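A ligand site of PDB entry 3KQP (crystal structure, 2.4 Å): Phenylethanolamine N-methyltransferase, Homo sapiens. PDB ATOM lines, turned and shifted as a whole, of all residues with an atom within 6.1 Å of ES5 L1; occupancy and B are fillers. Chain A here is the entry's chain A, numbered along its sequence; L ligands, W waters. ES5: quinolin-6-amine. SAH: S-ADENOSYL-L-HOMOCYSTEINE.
NZ of Lys 57 sits at hydrogen-bond distance from OH of Tyr 40 (2.9 Å). The side-chain amino group (NZ) of Lys 57 lies within hydrogen-bond range of the side-chain hydroxyl (OH) of Tyr 85, 2.9 Å away. The side-chain amide oxygen (OD1) of Asn 39 is in hydrogen-bond range of the guanidinium group (NH1) of Arg 44, 2.9 Å away. OD2 of Asp 267 lies within salt-bridge range of NH1 of Arg 44 (2.9 Å). N of Val 269 lies close to OD1 of Asp 267 (3.3 Å). OH of Tyr 85 is in hydrogen-bond range of OH of Tyr 40, 2.9 Å away.
OE1 of Glu 219 sits at hydrogen-bond distance from N01 of ES5 L1. NZ of Lys 57 sits at hydrogen-bond distance from N06 of ES5 L1 (3.1 Å). The side-chain hydroxyl (OH) of Tyr 35 sits at hydrogen-bond distance from an oxygen (OXT) of SAH L2 (2.7 Å). An oxygen (OXT) of SAH L2 sits at hydrogen-bond distance from the side-chain hydroxyl (OH) of Tyr 40 (2.6 Å). OH of Tyr 85 sits at hydrogen-bond distance from O of SAH L2 (2.7 Å).
Water W3 bridges N01 of ES5 L1 (2.8 Å) and O of Phe 182 (3.3 Å). Water W1 lies within hydrogen-bond range of OD2 of Asp 267, N01 of ES5 L1 and ND2 of Asn 39. Water W4 bridges O of Asn 39 (2.7 Å) and N06 of ES5 L1 (3.4 Å). Water W2 lies within hydrogen-bond range of the side-chain carboxylate (OE2) of Glu 219 (2.6 Å) and a nitrogen (N01) of ES5 L1 (3.4 Å).
OH of Tyr 35 touches C03 of ES5 L1, at 3.3 Å. Asn 39 touches ES5 L1 (OD1 to C10, 3.5 Å). Tyr 40 touches ES5 L1. Arg 44 touches ES5 L1. Val 53 touches ES5 L1 (CG2 to C07, 3.7 Å). Phe 182 touches ES5 L1 (CZ to N06, 3.3 Å). Tyr 222 touches ES5 L1 (CG to N01, 3.7 Å). Asp 267 touches ES5 L1. CG1 of Val 269 touches C09 of ES5 L1, 3.9 Å away. Val 272 touches ES5 L1. Hydrophobic or aromatic side chains within 4 Å of ES5 L1: Val 53, Phe 182, Tyr 222, Val 269 and Val 272. Within 4 Å of ES5 L1: Tyr 35, Asn 39, Tyr 40, Arg 44, Val 53, Lys 57, Phe 182, Glu 219, Tyr 222, Asp 267, Val 269 and Val 272.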
ATOM      1  N   TYR A  35     -23.988   2.292  17.656  1.00  0.00           N
ATOM      2  CA  TYR A  35     -23.974   3.742  17.678  1.00  0.00           C
ATOM      3  C   TYR A  35     -24.646   4.316  18.938  1.00  0.00           C
ATOM      4  O   TYR A  35     -24.125   5.253  19.547  1.00  0.00           O
ATOM      5  CB  TYR A  35     -24.627   4.298  16.421  1.00  0.00           C
ATOM      6  CG  TYR A  35     -24.801   5.798  16.417  1.00  0.00           C
ATOM      7  CD1 TYR A  35     -23.725   6.648  16.154  1.00  0.00           C
ATOM      8  CD2 TYR A  35     -26.045   6.378  16.670  1.00  0.00           C
ATOM      9  CE1 TYR A  35     -23.882   8.018  16.153  1.00  0.00           C
ATOM     10  CE2 TYR A  35     -26.212   7.746  16.665  1.00  0.00           C
ATOM     11  CZ  TYR A  35     -25.138   8.565  16.398  1.00  0.00           C
ATOM     12  OH  TYR A  35     -25.311   9.921  16.388  1.00  0.00           O
ATOM     13  N   ASN A  39     -22.650   6.524  21.863  1.00  0.00           N
ATOM     14  CA  ASN A  39     -22.980   7.931  22.067  1.00  0.00           C
ATOM     15  C   ASN A  39     -24.010   8.263  23.146  1.00  0.00           C
ATOM     16  O   ASN A  39     -23.996   9.351  23.722  1.00  0.00           O
ATOM     17  CB  ASN A  39     -23.383   8.578  20.747  1.00  0.00           C
ATOM     18  CG  ASN A  39     -22.186   8.937  19.880  1.00  0.00           C
ATOM     19  OD1 ASN A  39     -21.387   9.790  20.244  1.00  0.00           O
ATOM     20  ND2 ASN A  39     -22.068   8.272  18.746  1.00  0.00           N
ATOM     21  N   TYR A  40     -24.908   7.321  23.426  1.00  0.00           N
ATOM     22  CA  TYR A  40     -26.054   7.642  24.263  1.00  0.00           C
ATOM     23  C   TYR A  40     -26.165   6.765  25.503  1.00  0.00           C
ATOM     24  O   TYR A  40     -27.076   6.936  26.307  1.00  0.00           O
ATOM     25  CB  TYR A  40     -27.338   7.653  23.416  1.00  0.00           C
ATOM     26  CG  TYR A  40     -27.261   8.733  22.360  1.00  0.00           C
ATOM     27  CD1 TYR A  40     -26.836   8.441  21.066  1.00  0.00           C
ATOM     28  CD2 TYR A  40     -27.521  10.051  22.679  1.00  0.00           C
ATOM     29  CE1 TYR A  40     -26.729   9.443  20.109  1.00  0.00           C
ATOM     30  CE2 TYR A  40     -27.412  11.053  21.745  1.00  0.00           C
ATOM     31  CZ  TYR A  40     -27.022  10.753  20.458  1.00  0.00           C
ATOM     32  OH  TYR A  40     -26.925  11.773  19.543  1.00  0.00           O
ATOM     33  N   ARG A  44     -20.877   9.184  27.772  1.00  0.00           N
ATOM     34  CA  ARG A  44     -21.522  10.314  27.083  1.00  0.00           C
ATOM     35  C   ARG A  44     -23.006  10.355  27.373  1.00  0.00           C
ATOM     36  O   ARG A  44     -23.630  11.414  27.301  1.00  0.00           O
ATOM     37  CB  ARG A  44     -21.301  10.257  25.573  1.00  0.00           C
ATOM     38  CG  ARG A  44     -19.855  10.447  25.175  1.00  0.00           C
ATOM     39  CD  ARG A  44     -19.667  10.300  23.685  1.00  0.00           C
ATOM     40  NE  ARG A  44     -18.289  10.596  23.315  1.00  0.00           N
ATOM     41  CZ  ARG A  44     -17.871  10.783  22.074  1.00  0.00           C
ATOM     42  NH1 ARG A  44     -18.738  10.731  21.062  1.00  0.00           N
ATOM     43  NH2 ARG A  44     -16.595  11.042  21.833  1.00  0.00           N
ATOM     44  N   VAL A  53     -21.934  16.429  27.540  1.00  0.00           N
ATOM     45  CA  VAL A  53     -22.449  16.783  26.218  1.00  0.00           C
ATOM     46  C   VAL A  53     -23.932  16.496  26.048  1.00  0.00           C
ATOM     47  O   VAL A  53     -24.643  17.221  25.361  1.00  0.00           O
ATOM     48  CB  VAL A  53     -21.645  16.113  25.064  1.00  0.00           C
ATOM     49  CG1 VAL A  53     -21.936  14.611  24.990  1.00  0.00           C
ATOM     50  CG2 VAL A  53     -21.942  16.795  23.736  1.00  0.00           C
ATOM     51  N   GLY A  54     -24.410  15.426  26.686  1.00  0.00           N
ATOM     52  CA  GLY A  54     -25.818  15.102  26.672  1.00  0.00           C
ATOM     53  C   GLY A  54     -26.663  16.260  27.173  1.00  0.00           C
ATOM     54  O   GLY A  54     -27.495  16.804  26.449  1.00  0.00           O
ATOM     55  N   LYS A  57     -26.548  19.432  24.836  1.00  0.00           N
ATOM     56  CA  LYS A  57     -27.436  19.286  23.686  1.00  0.00           C
ATOM     57  C   LYS A  57     -28.910  19.502  24.043  1.00  0.00           C
ATOM     58  O   LYS A  57     -29.602  20.292  23.383  1.00  0.00           O
ATOM     59  CB  LYS A  57     -27.239  17.931  23.012  1.00  0.00           C
ATOM     60  CG  LYS A  57     -25.799  17.720  22.522  1.00  0.00           C
ATOM     61  CD  LYS A  57     -25.691  16.642  21.444  1.00  0.00           C
ATOM     62  CE  LYS A  57     -26.189  15.294  21.934  1.00  0.00           C
ATOM     63  NZ  LYS A  57     -26.110  14.249  20.881  1.00  0.00           N
ATOM     64  N   TYR A  85     -34.061  11.730  21.154  1.00  0.00           N
ATOM     65  CA  TYR A  85     -33.778  12.798  22.127  1.00  0.00           C
ATOM     66  C   TYR A  85     -33.913  14.168  21.496  1.00  0.00           C
ATOM     67  O   TYR A  85     -34.323  15.126  22.147  1.00  0.00           O
ATOM     68  CB  TYR A  85     -32.371  12.648  22.703  1.00  0.00           C
ATOM     69  CG  TYR A  85     -31.286  13.055  21.710  1.00  0.00           C
ATOM     70  CD1 TYR A  85     -30.797  14.349  21.687  1.00  0.00           C
ATOM     71  CD2 TYR A  85     -30.778  12.147  20.801  1.00  0.00           C
ATOM     72  CE1 TYR A  85     -29.819  14.730  20.778  1.00  0.00           C
ATOM     73  CE2 TYR A  85     -29.798  12.518  19.892  1.00  0.00           C
ATOM     74  CZ  TYR A  85     -29.325  13.808  19.883  1.00  0.00           C
ATOM     75  OH  TYR A  85     -28.364  14.185  18.989  1.00  0.00           O
ATOM     76  N   PHE A 182     -26.138  15.800  13.686  1.00  0.00           N
ATOM     77  CA  PHE A 182     -25.054  14.877  13.362  1.00  0.00           C
ATOM     78  C   PHE A 182     -25.290  14.104  12.074  1.00  0.00           C
ATOM     79  O   PHE A 182     -24.777  13.006  11.880  1.00  0.00           O
ATOM     80  CB  PHE A 182     -24.775  13.949  14.546  1.00  0.00           C
ATOM     81  CG  PHE A 182     -24.517  14.686  15.828  1.00  0.00           C
ATOM     82  CD1 PHE A 182     -25.538  14.890  16.743  1.00  0.00           C
ATOM     83  CD2 PHE A 182     -23.255  15.206  16.109  1.00  0.00           C
ATOM     84  CE1 PHE A 182     -25.305  15.583  17.924  1.00  0.00           C
ATOM     85  CE2 PHE A 182     -23.015  15.901  17.271  1.00  0.00           C
ATOM     86  CZ  PHE A 182     -24.046  16.093  18.192  1.00  0.00           C
ATOM     87  N   ALA A 186     -21.648  14.266   8.683  1.00  0.00           N
ATOM     88  CA  ALA A 186     -21.408  12.832   8.731  1.00  0.00           C
ATOM     89  C   ALA A 186     -21.743  12.098   7.420  1.00  0.00           C
ATOM     90  O   ALA A 186     -21.485  10.897   7.307  1.00  0.00           O
ATOM     91  CB  ALA A 186     -22.165  12.198   9.905  1.00  0.00           C
ATOM     92  N   ALA A 216     -21.068  17.527  14.868  1.00  0.00           N
ATOM     93  CA  ALA A 216     -19.718  17.405  15.381  1.00  0.00           C
ATOM     94  C   ALA A 216     -18.801  18.453  14.764  1.00  0.00           C
ATOM     95  O   ALA A 216     -18.909  18.764  13.577  1.00  0.00           O
ATOM     96  CB  ALA A 216     -19.191  16.024  15.118  1.00  0.00           C
ATOM     97  N   GLU A 219     -14.591  16.912  13.351  1.00  0.00           N
ATOM     98  CA  GLU A 219     -14.614  15.449  13.356  1.00  0.00           C
ATOM     99  C   GLU A 219     -14.252  14.919  11.967  1.00  0.00           C
ATOM    100  O   GLU A 219     -14.627  15.503  10.954  1.00  0.00           O
ATOM    101  CB  GLU A 219     -16.001  14.945  13.752  1.00  0.00           C
ATOM    102  CG  GLU A 219     -16.154  13.431  13.776  1.00  0.00           C
ATOM    103  CD  GLU A 219     -17.586  12.981  14.041  1.00  0.00           C
ATOM    104  OE1 GLU A 219     -17.811  12.038  14.827  1.00  0.00           O
ATOM    105  OE2 GLU A 219     -18.499  13.596  13.444  1.00  0.00           O
ATOM    106  N   TYR A 222     -16.121   8.456  12.628  1.00  0.00           N
ATOM    107  CA  TYR A 222     -16.711   7.840  13.815  1.00  0.00           C
ATOM    108  C   TYR A 222     -17.129   6.416  13.505  1.00  0.00           C
ATOM    109  O   TYR A 222     -17.300   6.056  12.345  1.00  0.00           O
ATOM    110  CB  TYR A 222     -17.887   8.654  14.361  1.00  0.00           C
ATOM    111  CG  TYR A 222     -19.166   8.542  13.568  1.00  0.00           C
ATOM    112  CD1 TYR A 222     -20.199   7.719  14.002  1.00  0.00           C
ATOM    113  CD2 TYR A 222     -19.362   9.275  12.394  1.00  0.00           C
ATOM    114  CE1 TYR A 222     -21.377   7.617  13.304  1.00  0.00           C
ATOM    115  CE2 TYR A 222     -20.547   9.182  11.683  1.00  0.00           C
ATOM    116  CZ  TYR A 222     -21.553   8.344  12.138  1.00  0.00           C
ATOM    117  OH  TYR A 222     -22.745   8.229  11.455  1.00  0.00           O
ATOM    118  N   MET A 258     -15.621  19.300  23.785  1.00  0.00           N
ATOM    119  CA  MET A 258     -15.652  17.935  24.307  1.00  0.00           C
ATOM    120  C   MET A 258     -14.571  17.718  25.374  1.00  0.00           C
ATOM    121  O   MET A 258     -13.377  17.754  25.074  1.00  0.00           O
ATOM    122  CB  MET A 258     -15.469  16.959  23.130  1.00  0.00           C
ATOM    123  CG  MET A 258     -15.984  15.541  23.356  1.00  0.00           C
ATOM    124  SD  MET A 258     -17.788  15.359  23.417  1.00  0.00           S
ATOM    125  CE  MET A 258     -18.327  16.895  22.688  1.00  0.00           C
ATOM    126  N   ASP A 267     -14.650   7.957  18.094  1.00  0.00           N
ATOM    127  CA  ASP A 267     -14.536   8.993  17.079  1.00  0.00           C
ATOM    128  C   ASP A 267     -13.418   9.961  17.442  1.00  0.00           C
ATOM    129  O   ASP A 267     -12.699   9.744  18.418  1.00  0.00           O
ATOM    130  CB  ASP A 267     -15.864   9.738  16.895  1.00  0.00           C
ATOM    131  CG  ASP A 267     -16.365  10.392  18.179  1.00  0.00           C
ATOM    132  OD1 ASP A 267     -15.549  10.942  18.947  1.00  0.00           O
ATOM    133  OD2 ASP A 267     -17.584  10.351  18.436  1.00  0.00           O
ATOM    134  N   VAL A 269     -14.196  13.507  17.456  1.00  0.00           N
ATOM    135  CA  VAL A 269     -14.916  14.776  17.554  1.00  0.00           C
ATOM    136  C   VAL A 269     -14.235  15.689  18.581  1.00  0.00           C
ATOM    137  O   VAL A 269     -13.849  15.239  19.657  1.00  0.00           O
ATOM    138  CB  VAL A 269     -16.386  14.541  17.926  1.00  0.00           C
ATOM    139  CG1 VAL A 269     -16.483  13.688  19.174  1.00  0.00           C
ATOM    140  CG2 VAL A 269     -17.106  15.868  18.150  1.00  0.00           C
ATOM    141  N   GLY A 271     -15.511  19.052  19.318  1.00  0.00           N
ATOM    142  CA  GLY A 271     -16.532  19.859  19.946  1.00  0.00           C
ATOM    143  C   GLY A 271     -17.865  19.660  19.272  1.00  0.00           C
ATOM    144  O   GLY A 271     -17.979  18.928  18.276  1.00  0.00           O
ATOM    145  N   VAL A 272     -18.900  20.301  19.811  1.00  0.00           N
ATOM    146  CA  VAL A 272     -20.226  20.183  19.236  1.00  0.00           C
ATOM    147  C   VAL A 272     -20.772  21.572  19.017  1.00  0.00           C
ATOM    148  O   VAL A 272     -20.657  22.440  19.889  1.00  0.00           O
ATOM    149  CB  VAL A 272     -21.183  19.406  20.172  1.00  0.00           C
ATOM    150  CG1 VAL A 272     -22.608  19.449  19.642  1.00  0.00           C
ATOM    151  CG2 VAL A 272     -20.697  17.964  20.351  1.00  0.00           C
HETATM  152  C10 ES5 L   1     -21.125  13.012  18.946  1.00  0.00           C
HETATM  153  N01 ES5 L   1     -20.675  11.173  15.653  1.00  0.00           N
HETATM  154  C02 ES5 L   1     -21.296  11.792  16.820  1.00  0.00           C
HETATM  155  C03 ES5 L   1     -22.711  11.801  16.939  1.00  0.00           C
HETATM  156  C04 ES5 L   1     -23.331  12.401  18.060  1.00  0.00           C
HETATM  157  C05 ES5 L   1     -22.529  13.025  19.059  1.00  0.00           C
HETATM  158  N06 ES5 L   1     -23.135  13.618  20.153  1.00  0.00           N
HETATM  159  C07 ES5 L   1     -22.360  14.215  21.126  1.00  0.00           C
HETATM  160  C08 ES5 L   1     -20.954  14.213  21.026  1.00  0.00           C
HETATM  161  C09 ES5 L   1     -20.346  13.610  19.932  1.00  0.00           C
HETATM  162  C11 ES5 L   1     -20.504  12.402  17.823  1.00  0.00           C
HETATM  163  N   SAH L   2     -29.882  12.344  14.327  1.00  0.00           N
HETATM  164  CA  SAH L   2     -29.010  11.370  14.973  1.00  0.00           C
HETATM  165  CB  SAH L   2     -27.749  11.240  14.107  1.00  0.00           C
HETATM  166  CG  SAH L   2     -27.671   9.825  13.509  1.00  0.00           C
HETATM  167  SD  SAH L   2     -25.989   9.633  12.858  1.00  0.00           S
HETATM  168  C   SAH L   2     -28.583  11.908  16.353  1.00  0.00           C
HETATM  169  O   SAH L   2     -28.773  13.048  16.626  1.00  0.00           O
HETATM  170  OXT SAH L   2     -27.592  11.206  17.046  1.00  0.00           O
HETATM  171  C5' SAH L   2     -25.943  10.158  11.118  1.00  0.00           C
HETATM  172  C4' SAH L   2     -27.220   9.685  10.403  1.00  0.00           C
HETATM  173  O4' SAH L   2     -27.207  10.101   9.005  1.00  0.00           O
HETATM  174  C3' SAH L   2     -27.358   8.144  10.407  1.00  0.00           C
HETATM  175  O3' SAH L   2     -28.618   7.780  10.902  1.00  0.00           O
HETATM  176  C2' SAH L   2     -27.241   7.816   8.943  1.00  0.00           C
HETATM  177  O2' SAH L   2     -27.823   6.592   8.548  1.00  0.00           O
HETATM  178  C1' SAH L   2     -27.884   9.028   8.286  1.00  0.00           C
HETATM  179  N9  SAH L   2     -27.502   9.067   6.894  1.00  0.00           N
HETATM  180  C8  SAH L   2     -26.387   8.292   6.264  1.00  0.00           C
HETATM  181  N7  SAH L   2     -26.339   8.655   4.863  1.00  0.00           N
HETATM  182  C5  SAH L   2     -27.394   9.650   4.612  1.00  0.00           C
HETATM  183  C6  SAH L   2     -27.795  10.367   3.355  1.00  0.00           C
HETATM  184  N6  SAH L   2     -27.061  10.114   2.124  1.00  0.00           N
HETATM  185  N1  SAH L   2     -28.902  11.322   3.404  1.00  0.00           N
HETATM  186  C2  SAH L   2     -29.637  11.584   4.689  1.00  0.00           C
HETATM  187  N3  SAH L   2     -29.240  10.855   5.932  1.00  0.00           N
HETATM  188  C4  SAH L   2     -28.120   9.904   5.879  1.00  0.00           C
HETATM  189  O   HOH W   1     -19.590   9.013  17.275  1.00  0.00           O
HETATM  190  O   HOH W   2     -21.053  13.654  13.397  1.00  0.00           O
HETATM  191  O   HOH W   3     -22.389  11.374  13.423  1.00  0.00           O
HETATM  192  O   HOH W   4     -22.731  11.634  22.899  1.00  0.00           O
